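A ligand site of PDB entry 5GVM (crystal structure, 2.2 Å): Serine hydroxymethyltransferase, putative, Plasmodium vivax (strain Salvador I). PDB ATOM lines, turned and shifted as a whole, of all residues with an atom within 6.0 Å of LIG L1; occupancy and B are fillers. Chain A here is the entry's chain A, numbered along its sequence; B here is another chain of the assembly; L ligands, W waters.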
ATOM      1  N   HIS A 123       7.221  -0.916 -10.021  1.00  0.00           N
ATOM      2  CA  HIS A 123       7.393  -2.028  -9.092  1.00  0.00           C
ATOM      3  C   HIS A 123       7.864  -1.494  -7.731  1.00  0.00           C
ATOM      4  O   HIS A 123       8.620  -0.499  -7.660  1.00  0.00           O
ATOM      5  CB  HIS A 123       8.379  -3.029  -9.680  1.00  0.00           C
ATOM      6  CG  HIS A 123       8.375  -4.369  -9.008  1.00  0.00           C
ATOM      7  ND1 HIS A 123       9.001  -4.575  -7.805  1.00  0.00           N
ATOM      8  CD2 HIS A 123       7.847  -5.562  -9.370  1.00  0.00           C
ATOM      9  CE1 HIS A 123       8.843  -5.838  -7.445  1.00  0.00           C
ATOM     10  NE2 HIS A 123       8.151  -6.462  -8.386  1.00  0.00           N
ATOM     11  N   LEU A 124       7.422  -2.173  -6.665  1.00  0.00           N
ATOM     12  CA  LEU A 124       7.742  -1.819  -5.265  1.00  0.00           C
ATOM     13  C   LEU A 124       9.243  -1.644  -5.009  1.00  0.00           C
ATOM     14  O   LEU A 124       9.679  -0.607  -4.497  1.00  0.00           O
ATOM     15  CB  LEU A 124       7.145  -2.879  -4.317  1.00  0.00           C
ATOM     16  CG  LEU A 124       7.257  -2.716  -2.787  1.00  0.00           C
ATOM     17  CD1 LEU A 124       6.410  -1.560  -2.287  1.00  0.00           C
ATOM     18  CD2 LEU A 124       6.829  -3.989  -2.085  1.00  0.00           C
ATOM     19  N   CYS A 125      10.000  -2.678  -5.341  1.00  0.00           N
ATOM     20  CA  CYS A 125      11.491  -2.682  -5.364  1.00  0.00           C
ATOM     21  C   CYS A 125      12.168  -1.563  -6.117  1.00  0.00           C
ATOM     22  O   CYS A 125      13.315  -1.224  -5.808  1.00  0.00           O
ATOM     23  CB  CYS A 125      12.018  -4.009  -5.947  1.00  0.00           C
ATOM     24  SG  CYS A 125      11.827  -5.433  -4.840  1.00  0.00           S
ATOM     25  N   SER A 126      11.501  -1.009  -7.133  1.00  0.00           N
ATOM     26  CA  SER A 126      12.036   0.109  -7.910  1.00  0.00           C
ATOM     27  C   SER A 126      11.611   1.489  -7.394  1.00  0.00           C
ATOM     28  O   SER A 126      12.001   2.500  -7.977  1.00  0.00           O
ATOM     29  CB  SER A 126      11.614  -0.058  -9.358  1.00  0.00           C
ATOM     30  OG  SER A 126      12.115  -1.286  -9.889  1.00  0.00           O
ATOM     31  N   GLY A 127      10.815   1.535  -6.335  1.00  0.00           N
ATOM     32  CA  GLY A 127      10.362   2.791  -5.732  1.00  0.00           C
ATOM     33  C   GLY A 127       8.878   3.058  -5.829  1.00  0.00           C
ATOM     34  O   GLY A 127       8.422   4.091  -5.347  1.00  0.00           O
ATOM     35  N   GLY A 128       8.102   2.132  -6.409  1.00  0.00           N
ATOM     36  CA  GLY A 128       6.649   2.290  -6.499  1.00  0.00           C
ATOM     37  C   GLY A 128       5.893   1.982  -5.211  1.00  0.00           C
ATOM     38  O   GLY A 128       6.399   1.288  -4.338  1.00  0.00           O
ATOM     39  N   HIS A 129       4.687   2.527  -5.077  1.00  0.00           N
ATOM     40  CA  HIS A 129       3.841   2.196  -3.934  1.00  0.00           C
ATOM     41  C   HIS A 129       3.124   0.846  -4.051  1.00  0.00           C
ATOM     42  O   HIS A 129       2.924   0.331  -5.136  1.00  0.00           O
ATOM     43  CB  HIS A 129       2.816   3.301  -3.651  1.00  0.00           C
ATOM     44  CG  HIS A 129       2.244   3.231  -2.259  1.00  0.00           C
ATOM     45  ND1 HIS A 129       0.914   3.022  -2.017  1.00  0.00           N
ATOM     46  CD2 HIS A 129       2.853   3.246  -1.052  1.00  0.00           C
ATOM     47  CE1 HIS A 129       0.703   2.947  -0.715  1.00  0.00           C
ATOM     48  NE2 HIS A 129       1.876   3.080  -0.110  1.00  0.00           N
ATOM     49  N   LEU A 130       2.755   0.289  -2.910  1.00  0.00           N
ATOM     50  CA  LEU A 130       1.900  -0.904  -2.833  1.00  0.00           C
ATOM     51  C   LEU A 130       0.634  -0.769  -3.658  1.00  0.00           C
ATOM     52  O   LEU A 130       0.257  -1.716  -4.343  1.00  0.00           O
ATOM     53  CB  LEU A 130       1.514  -1.230  -1.376  1.00  0.00           C
ATOM     54  CG  LEU A 130       2.652  -1.715  -0.479  1.00  0.00           C
ATOM     55  CD1 LEU A 130       2.160  -1.900   0.937  1.00  0.00           C
ATOM     56  CD2 LEU A 130       3.254  -3.022  -0.969  1.00  0.00           C
ATOM     57  N   PHE A 134       0.996  -3.626  -6.809  1.00  0.00           N
ATOM     58  CA  PHE A 134       2.058  -4.517  -6.359  1.00  0.00           C
ATOM     59  C   PHE A 134       1.606  -5.945  -6.099  1.00  0.00           C
ATOM     60  O   PHE A 134       0.614  -6.172  -5.383  1.00  0.00           O
ATOM     61  CB  PHE A 134       2.768  -4.006  -5.121  1.00  0.00           C
ATOM     62  CG  PHE A 134       3.801  -4.962  -4.608  1.00  0.00           C
ATOM     63  CD1 PHE A 134       4.948  -5.248  -5.372  1.00  0.00           C
ATOM     64  CD2 PHE A 134       3.616  -5.638  -3.399  1.00  0.00           C
ATOM     65  CE1 PHE A 134       5.886  -6.160  -4.925  1.00  0.00           C
ATOM     66  CE2 PHE A 134       4.564  -6.558  -2.957  1.00  0.00           C
ATOM     67  CZ  PHE A 134       5.699  -6.814  -3.719  1.00  0.00           C
ATOM     68  N   ASP A 136       3.606 -10.300  -6.114  1.00  0.00           N
ATOM     69  CA  ASP A 136       4.798 -11.150  -6.283  1.00  0.00           C
ATOM     70  C   ASP A 136       4.398 -12.529  -6.847  1.00  0.00           C
ATOM     71  O   ASP A 136       3.208 -12.827  -7.030  1.00  0.00           O
ATOM     72  CB  ASP A 136       5.621 -11.247  -4.970  1.00  0.00           C
ATOM     73  CG  ASP A 136       5.143 -12.342  -4.015  1.00  0.00           C
ATOM     74  OD1 ASP A 136       3.954 -12.729  -3.999  1.00  0.00           O
ATOM     75  OD2 ASP A 136       5.999 -12.835  -3.245  1.00  0.00           O
ATOM     76  N   VAL A 141      -0.391  -9.139  -3.363  1.00  0.00           N
ATOM     77  CA  VAL A 141      -0.115  -8.495  -2.069  1.00  0.00           C
ATOM     78  C   VAL A 141      -1.031  -7.284  -1.848  1.00  0.00           C
ATOM     79  O   VAL A 141      -1.538  -7.068  -0.740  1.00  0.00           O
ATOM     80  CB  VAL A 141       1.374  -8.054  -2.004  1.00  0.00           C
ATOM     81  CG1 VAL A 141       1.667  -7.207  -0.777  1.00  0.00           C
ATOM     82  CG2 VAL A 141       2.287  -9.271  -2.050  1.00  0.00           C
ATOM     83  N   THR A 183       7.091   6.264  -4.130  1.00  0.00           N
ATOM     84  CA  THR A 183       7.330   6.349  -2.654  1.00  0.00           C
ATOM     85  C   THR A 183       8.801   6.497  -2.288  1.00  0.00           C
ATOM     86  O   THR A 183       9.124   7.276  -1.392  1.00  0.00           O
ATOM     87  CB  THR A 183       6.679   5.220  -1.813  1.00  0.00           C
ATOM     88  OG1 THR A 183       7.656   4.360  -1.205  1.00  0.00           O
ATOM     89  CG2 THR A 183       5.759   4.414  -2.616  1.00  0.00           C
ATOM     90  N   SER A 184       9.670   5.768  -2.989  1.00  0.00           N
ATOM     91  CA  SER A 184      11.116   5.771  -2.721  1.00  0.00           C
ATOM     92  C   SER A 184      11.922   6.098  -3.974  1.00  0.00           C
ATOM     93  O   SER A 184      12.994   5.528  -4.186  1.00  0.00           O
ATOM     94  CB  SER A 184      11.530   4.403  -2.163  1.00  0.00           C
ATOM     95  OG  SER A 184      10.647   4.026  -1.135  1.00  0.00           O
ATOM     96  N   ASN A 354      13.787   4.176   7.495  1.00  0.00           N
ATOM     97  CA  ASN A 354      13.294   2.875   7.107  1.00  0.00           C
ATOM     98  C   ASN A 354      14.216   2.129   6.176  1.00  0.00           C
ATOM     99  O   ASN A 354      14.944   2.737   5.373  1.00  0.00           O
ATOM    100  CB  ASN A 354      11.862   2.956   6.534  1.00  0.00           C
ATOM    101  CG  ASN A 354      11.795   3.690   5.223  1.00  0.00           C
ATOM    102  OD1 ASN A 354      11.581   4.895   5.197  1.00  0.00           O
ATOM    103  ND2 ASN A 354      11.984   2.975   4.127  1.00  0.00           N
ATOM    104  N   LYS A 355      14.179   0.813   6.316  1.00  0.00           N
ATOM    105  CA  LYS A 355      14.789  -0.093   5.368  1.00  0.00           C
ATOM    106  C   LYS A 355      14.100   0.034   4.025  1.00  0.00           C
ATOM    107  O   LYS A 355      12.907   0.346   3.943  1.00  0.00           O
ATOM    108  CB  LYS A 355      14.774  -1.557   5.847  1.00  0.00           C
ATOM    109  CG  LYS A 355      13.508  -2.031   6.550  1.00  0.00           C
ATOM    110  CD  LYS A 355      13.341  -3.540   6.454  1.00  0.00           C
ATOM    111  CE  LYS A 355      12.414  -4.064   7.544  1.00  0.00           C
ATOM    112  NZ  LYS A 355      11.445  -5.054   7.000  1.00  0.00           N
ATOM    113  N   ASN A 356      14.858  -0.189   2.960  1.00  0.00           N
ATOM    114  CA  ASN A 356      14.343   0.104   1.622  1.00  0.00           C
ATOM    115  C   ASN A 356      15.111  -0.726   0.631  1.00  0.00           C
ATOM    116  O   ASN A 356      16.301  -0.922   0.776  1.00  0.00           O
ATOM    117  CB  ASN A 356      14.485   1.594   1.311  1.00  0.00           C
ATOM    118  CG  ASN A 356      13.413   2.098   0.357  1.00  0.00           C
ATOM    119  OD1 ASN A 356      12.405   2.673   0.772  1.00  0.00           O
ATOM    120  ND2 ASN A 356      13.622   1.861  -0.932  1.00  0.00           N
ATOM    121  N   THR A 357      14.412  -1.222  -0.374  1.00  0.00           N
ATOM    122  CA  THR A 357      15.066  -1.909  -1.469  1.00  0.00           C
ATOM    123  C   THR A 357      15.927  -0.985  -2.334  1.00  0.00           C
ATOM    124  O   THR A 357      15.848   0.269  -2.230  1.00  0.00           O
ATOM    125  CB  THR A 357      14.021  -2.533  -2.369  1.00  0.00           C
ATOM    126  OG1 THR A 357      13.094  -1.512  -2.705  1.00  0.00           O
ATOM    127  CG2 THR A 357      13.320  -3.695  -1.645  1.00  0.00           C
ATOM    128  N   ASP A 363      14.925  -9.944  -3.129  1.00  0.00           N
ATOM    129  CA  ASP A 363      14.017 -10.245  -2.013  1.00  0.00           C
ATOM    130  C   ASP A 363      13.843  -9.027  -1.089  1.00  0.00           C
ATOM    131  O   ASP A 363      14.821  -8.366  -0.727  1.00  0.00           O
ATOM    132  CB  ASP A 363      14.551 -11.393  -1.140  1.00  0.00           C
ATOM    133  CG  ASP A 363      15.045 -12.578  -1.950  1.00  0.00           C
ATOM    134  OD1 ASP A 363      16.198 -12.518  -2.432  1.00  0.00           O
ATOM    135  OD2 ASP A 363      14.284 -13.576  -2.076  1.00  0.00           O
ATOM    136  N   CYS A 364      12.596  -8.769  -0.700  1.00  0.00           N
ATOM    137  CA  CYS A 364      12.289  -7.816   0.381  1.00  0.00           C
ATOM    138  C   CYS A 364      12.561  -8.389   1.773  1.00  0.00           C
ATOM    139  O   CYS A 364      12.382  -7.697   2.781  1.00  0.00           O
ATOM    140  CB  CYS A 364      10.837  -7.355   0.274  1.00  0.00           C
ATOM    141  SG  CYS A 364      10.443  -6.635  -1.328  1.00  0.00           S
ATOM    142  N   VAL A 365      12.956  -9.669   1.828  1.00  0.00           N
ATOM    143  CA  VAL A 365      13.411 -10.289   3.072  1.00  0.00           C
ATOM    144  C   VAL A 365      14.740  -9.661   3.492  1.00  0.00           C
ATOM    145  O   VAL A 365      14.977  -9.470   4.686  1.00  0.00           O
ATOM    146  CB  VAL A 365      13.590 -11.834   2.981  1.00  0.00           C
ATOM    147  CG1 VAL A 365      13.567 -12.441   4.384  1.00  0.00           C
ATOM    148  CG2 VAL A 365      12.524 -12.508   2.102  1.00  0.00           C
ATOM    149  N   PRO A 367      16.473  -6.305   2.355  1.00  0.00           N
ATOM    150  CA  PRO A 367      16.694  -5.067   1.604  1.00  0.00           C
ATOM    151  C   PRO A 367      18.090  -4.490   1.832  1.00  0.00           C
ATOM    152  O   PRO A 367      18.584  -4.480   2.963  1.00  0.00           O
ATOM    153  CB  PRO A 367      15.616  -4.123   2.145  1.00  0.00           C
ATOM    154  CG  PRO A 367      15.356  -4.612   3.518  1.00  0.00           C
ATOM    155  CD  PRO A 367      15.508  -6.112   3.450  1.00  0.00           C
ATOM    156  N   GLY A 369      19.228  -1.321   1.316  1.00  0.00           N
ATOM    157  CA  GLY A 369      19.369   0.098   1.554  1.00  0.00           C
ATOM    158  C   GLY A 369      18.472   0.627   2.623  1.00  0.00           C
ATOM    159  O   GLY A 369      17.651  -0.081   3.166  1.00  0.00           O
ATOM    160  N   ARG A 371      16.089   4.300   3.157  1.00  0.00           N
ATOM    161  CA  ARG A 371      15.621   5.557   2.676  1.00  0.00           C
ATOM    162  C   ARG A 371      15.645   6.554   3.837  1.00  0.00           C
ATOM    163  O   ARG A 371      15.277   6.211   4.974  1.00  0.00           O
ATOM    164  CB  ARG A 371      14.219   5.415   2.104  1.00  0.00           C
ATOM    165  CG  ARG A 371      13.579   6.710   1.611  1.00  0.00           C
ATOM    166  CD  ARG A 371      12.118   6.510   1.301  1.00  0.00           C
ATOM    167  NE  ARG A 371      11.315   6.406   2.520  1.00  0.00           N
ATOM    168  CZ  ARG A 371       9.980   6.406   2.582  1.00  0.00           C
ATOM    169  NH1 ARG A 371       9.241   6.499   1.463  1.00  0.00           N
ATOM    170  NH2 ARG A 371       9.397   6.310   3.770  1.00  0.00           N
ATOM    171  N   GLU B  56       3.293   1.343   9.468  1.00  0.00           N
ATOM    172  CA  GLU B  56       2.703   0.307   8.618  1.00  0.00           C
ATOM    173  C   GLU B  56       3.105  -1.082   9.084  1.00  0.00           C
ATOM    174  O   GLU B  56       4.262  -1.297   9.409  1.00  0.00           O
ATOM    175  CB  GLU B  56       3.102   0.448   7.149  1.00  0.00           C
ATOM    176  CG  GLU B  56       2.771   1.807   6.551  1.00  0.00           C
ATOM    177  CD  GLU B  56       2.897   1.875   5.052  1.00  0.00           C
ATOM    178  OE1 GLU B  56       3.190   0.857   4.436  1.00  0.00           O
ATOM    179  OE2 GLU B  56       2.670   2.960   4.482  1.00  0.00           O
ATOM    180  N   TYR B  63       7.668  -1.552   9.425  1.00  0.00           N
ATOM    181  CA  TYR B  63       8.548  -1.083   8.375  1.00  0.00           C
ATOM    182  C   TYR B  63       9.221   0.278   8.674  1.00  0.00           C
ATOM    183  O   TYR B  63       9.939   0.791   7.809  1.00  0.00           O
ATOM    184  CB  TYR B  63       7.787  -1.016   7.055  1.00  0.00           C
ATOM    185  CG  TYR B  63       7.374  -2.384   6.521  1.00  0.00           C
ATOM    186  CD1 TYR B  63       6.196  -2.982   6.935  1.00  0.00           C
ATOM    187  CD2 TYR B  63       8.173  -3.064   5.616  1.00  0.00           C
ATOM    188  CE1 TYR B  63       5.827  -4.220   6.454  1.00  0.00           C
ATOM    189  CE2 TYR B  63       7.807  -4.315   5.142  1.00  0.00           C
ATOM    190  CZ  TYR B  63       6.639  -4.892   5.559  1.00  0.00           C
ATOM    191  OH  TYR B  63       6.280  -6.130   5.076  1.00  0.00           O
ATOM    192  N   TYR B  64       8.979   0.883   9.847  1.00  0.00           N
ATOM    193  CA  TYR B  64       9.681   2.125  10.217  1.00  0.00           C
ATOM    194  C   TYR B  64      10.306   2.036  11.603  1.00  0.00           C
ATOM    195  O   TYR B  64       9.854   1.290  12.495  1.00  0.00           O
ATOM    196  CB  TYR B  64       8.749   3.369  10.124  1.00  0.00           C
ATOM    197  CG  TYR B  64       8.078   3.440   8.789  1.00  0.00           C
ATOM    198  CD1 TYR B  64       6.888   2.765   8.564  1.00  0.00           C
ATOM    199  CD2 TYR B  64       8.653   4.129   7.720  1.00  0.00           C
ATOM    200  CE1 TYR B  64       6.269   2.791   7.330  1.00  0.00           C
ATOM    201  CE2 TYR B  64       8.050   4.150   6.469  1.00  0.00           C
ATOM    202  CZ  TYR B  64       6.859   3.484   6.280  1.00  0.00           C
ATOM    203  OH  TYR B  64       6.216   3.501   5.072  1.00  0.00           O
ATOM    204  N   PHE B 266      -3.917  -4.713   6.147  1.00  0.00           N
ATOM    205  CA  PHE B 266      -2.633  -4.304   5.570  1.00  0.00           C
ATOM    206  C   PHE B 266      -1.811  -5.522   5.188  1.00  0.00           C
ATOM    207  O   PHE B 266      -1.669  -6.416   6.003  1.00  0.00           O
ATOM    208  CB  PHE B 266      -1.836  -3.451   6.548  1.00  0.00           C
ATOM    209  CG  PHE B 266      -0.445  -3.169   6.093  1.00  0.00           C
ATOM    210  CD1 PHE B 266      -0.186  -2.097   5.240  1.00  0.00           C
ATOM    211  CD2 PHE B 266       0.622  -4.002   6.463  1.00  0.00           C
ATOM    212  CE1 PHE B 266       1.093  -1.836   4.790  1.00  0.00           C
ATOM    213  CE2 PHE B 266       1.911  -3.740   6.009  1.00  0.00           C
ATOM    214  CZ  PHE B 266       2.141  -2.661   5.168  1.00  0.00           C
ATOM    215  N   PRO B 267      -1.186  -5.535   4.005  1.00  0.00           N
ATOM    216  CA  PRO B 267      -1.062  -4.511   2.989  1.00  0.00           C
ATOM    217  C   PRO B 267      -2.079  -4.563   1.838  1.00  0.00           C
ATOM    218  O   PRO B 267      -1.876  -3.839   0.860  1.00  0.00           O
ATOM    219  CB  PRO B 267       0.350  -4.778   2.438  1.00  0.00           C
ATOM    220  CG  PRO B 267       0.453  -6.258   2.469  1.00  0.00           C
ATOM    221  CD  PRO B 267      -0.272  -6.671   3.722  1.00  0.00           C
HETATM  222  O1  LIG L   1       7.520  -9.889   0.435  1.00  0.00           O
HETATM  223  C1  LIG L   1       6.965  -8.956   1.057  1.00  0.00           C
HETATM  224  O2  LIG L   1       7.149  -8.775   2.285  1.00  0.00           O
HETATM  225  C2  LIG L   1       6.050  -8.017   0.282  1.00  0.00           C
HETATM  226  C3  LIG L   1       5.864  -6.711   1.041  1.00  0.00           C
HETATM  227  C4  LIG L   1       6.892  -5.753   1.028  1.00  0.00           C
HETATM  228  C5  LIG L   1       4.690  -6.482   1.728  1.00  0.00           C
HETATM  229  C6  LIG L   1       4.545  -5.299   2.443  1.00  0.00           C
HETATM  230  C7  LIG L   1       5.563  -4.333   2.436  1.00  0.00           C
HETATM  231  C8  LIG L   1       6.726  -4.549   1.713  1.00  0.00           C
HETATM  232  C9  LIG L   1       7.794  -3.516   1.758  1.00  0.00           C
HETATM  233  C10 LIG L   1       9.070  -3.932   2.109  1.00  0.00           C
HETATM  234  C11 LIG L   1      10.104  -3.007   2.226  1.00  0.00           C
HETATM  235  C12 LIG L   1      11.485  -3.466   2.607  1.00  0.00           C
HETATM  236  F1  LIG L   1      12.391  -2.530   2.601  1.00  0.00           F
HETATM  237  F2  LIG L   1      11.398  -4.039   3.789  1.00  0.00           F
HETATM  238  F3  LIG L   1      11.929  -4.308   1.721  1.00  0.00           F
HETATM  239  C13 LIG L   1       9.854  -1.658   1.996  1.00  0.00           C
HETATM  240  C14 LIG L   1       7.541  -2.164   1.519  1.00  0.00           C
HETATM  241  C15 LIG L   1       8.576  -1.201   1.649  1.00  0.00           C
HETATM  242  C16 LIG L   1       8.373   0.283   1.331  1.00  0.00           C
HETATM  243  C17 LIG L   1       9.125   1.299   2.235  1.00  0.00           C
HETATM  244  C18 LIG L   1       8.806   2.769   1.903  1.00  0.00           C
HETATM  245  C19 LIG L   1       8.976   1.076   3.754  1.00  0.00           C
HETATM  246  C20 LIG L   1       8.919   0.419  -0.096  1.00  0.00           C
HETATM  247  C21 LIG L   1      10.088   0.032  -0.352  1.00  0.00           C
HETATM  248  N1  LIG L   1      11.165  -0.329  -0.560  1.00  0.00           N
HETATM  249  C22 LIG L   1       8.217   0.938  -1.135  1.00  0.00           C
HETATM  250  N2  LIG L   1       8.691   1.052  -2.373  1.00  0.00           N
HETATM  251  C23 LIG L   1       6.920   0.592   1.326  1.00  0.00           C
HETATM  252  C24 LIG L   1       5.818   0.424   2.305  1.00  0.00           C
HETATM  253  C25 LIG L   1       5.882  -0.109   3.708  1.00  0.00           C
HETATM  254  N3  LIG L   1       4.706   0.859   1.680  1.00  0.00           N
HETATM  255  N4  LIG L   1       4.912   1.270   0.351  1.00  0.00           N
HETATM  256  C26 LIG L   1       6.207   1.110   0.169  1.00  0.00           C
HETATM  257  O3  LIG L   1       6.871   1.399  -0.966  1.00  0.00           O
HETATM  258  N1  LG2 L   2       1.118   7.100  -2.356  1.00  0.00           N
HETATM  259  C1  LG2 L   2       2.448   7.158  -2.188  1.00  0.00           C
HETATM  260  C2  LG2 L   2       3.378   7.632  -3.284  1.00  0.00           C
HETATM  261  C3  LG2 L   2       2.980   6.733  -0.867  1.00  0.00           C
HETATM  262  O1  LG2 L   2       4.290   6.799  -0.657  1.00  0.00           O
HETATM  263  C4  LG2 L   2       2.062   6.271   0.197  1.00  0.00           C
HETATM  264  C5  LG2 L   2       2.534   5.850   1.570  1.00  0.00           C
HETATM  265  C6  LG2 L   2       0.621   6.267  -0.128  1.00  0.00           C
HETATM  266  C7  LG2 L   2       0.246   6.669  -1.417  1.00  0.00           C
HETATM  267  C8  LG2 L   2      -0.406   5.784   0.874  1.00  0.00           C
HETATM  268  O2  LG2 L   2      -0.633   6.651   1.989  1.00  0.00           O
HETATM  269  P1  LG2 L   2      -1.321   6.081   3.331  1.00  0.00           P
HETATM  270  O3  LG2 L   2      -0.160   5.430   4.032  1.00  0.00           O
HETATM  271  O4  LG2 L   2      -2.349   5.062   2.905  1.00  0.00           O
HETATM  272  O5  LG2 L   2      -1.819   7.349   3.963  1.00  0.00           O
HETATM  273  C9  LG2 L   2       6.074   5.746   2.809  1.00  0.00           C
HETATM  274  O6  LG2 L   2       6.628   6.414   1.925  1.00  0.00           O
HETATM  275  O7  LG2 L   2       6.537   5.659   3.948  1.00  0.00           O
HETATM  276  C10 LG2 L   2       4.763   5.068   2.443  1.00  0.00           C
HETATM  277  N2  LG2 L   2       3.950   6.042   1.748  1.00  0.00           N
HETATM  278  O   HOH W   1      11.731   1.024  -3.135  1.00  0.00           O
HETATM  279  O   HOH W   2       1.994   1.075   1.946  1.00  0.00           O
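A fluorine (F1) of LIG L1 sits close to the backbone carbonyl oxygen (O) of Lys 355 (3.2 Å).
Residues that only touch LIG L1: His 129, Leu 130, Phe 134, Val 141, Ser 184, Asn 354, Cys 364, Pro 367, Arg 371, Tyr 63 of chain B and Tyr 64 of chain B.
18 residues have an atom within 4 Å of LIG L1: Leu 124, Gly 128, His 129, Leu 130, Phe 134, Val 141, Thr 183, Ser 184, Asn 354, Lys 355, Asn 356, Thr 357, Cys 364, Pro 367, Arg 371, Glu 56 of chain B, Tyr 63 of chain B and Tyr 64 of chain B.
An oxygen (O3) of LIG L1 sits at hydrogen-bond distance from the side-chain hydroxyl of Thr 183 (3.1 Å).
N3 of LIG L1 sits close to OE1 of Glu 56 of chain B.
O6 of LG2 L2 lies within salt-bridge range of NH1 of Arg 371 (2.7 Å).
ND2 of Asn 356 lies within hydrogen-bond range of N1 of LIG L1.
The side-chain hydroxyl of Thr 357 is in hydrogen-bond range of a nitrogen (N1) of LIG L1, 3.1 Å away.
O of Gly 128 lies within hydrogen-bond range of N2 of LIG L1 (3.0 Å).
The side-chain hydroxyl of Tyr 64 of chain B is in hydrogen-bond range of an oxygen (O7) of LG2 L2, at 2.5 Å.
N1 of LIG L1 lies within hydrogen-bond range of N of Thr 357, at 3.4 Å.
A nitrogen (N2) of LIG L1 sits at hydrogen-bond distance from the backbone carbonyl oxygen (O) of Leu 124 (2.9 Å).
O of Thr 183 sits at hydrogen-bond distance from NH1 of Arg 371, at 3.0 Å.
The backbone carbonyl oxygen of Glu 56 of chain B is in hydrogen-bond range of the backbone NH of Tyr 63 of chain B, 3.4 Å away.
OG1 of Thr 183 lies within hydrogen-bond range of OG of Ser 184, 3.0 Å away.
The backbone NH of Gly 128 is in hydrogen-bond range of the backbone carbonyl oxygen of His 123 (3.0 Å).
OD1 of Asn 356 sits at hydrogen-bond distance from OG of Ser 184.
The backbone carbonyl oxygen (O) of Gly 127 sits at hydrogen-bond distance from the backbone NH (N) of Ser 184 (3.2 Å).
The side-chain amide nitrogen (ND2) of Asn 354 lies within hydrogen-bond range of the side-chain amide oxygen (OD1) of Asn 356, at 3.4 Å.
OG1 of Thr 357 sits at hydrogen-bond distance from O of Cys 125 (3.1 Å).
Water W2 lies within hydrogen-bond range of N3 of LIG L1 (2.7 Å), OE1 of Glu 56 of chain B (2.8 Å) and NE2 of His 129 (2.9 Å).
Water W1 lies within hydrogen-bond range of OG1 of Thr 357 (2.9 Å), O of Leu 124 (3.0 Å), N1 of LIG L1 (3.0 Å), ND2 of Asn 356 (3.0 Å) and N of Gly 127 (3.4 Å).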
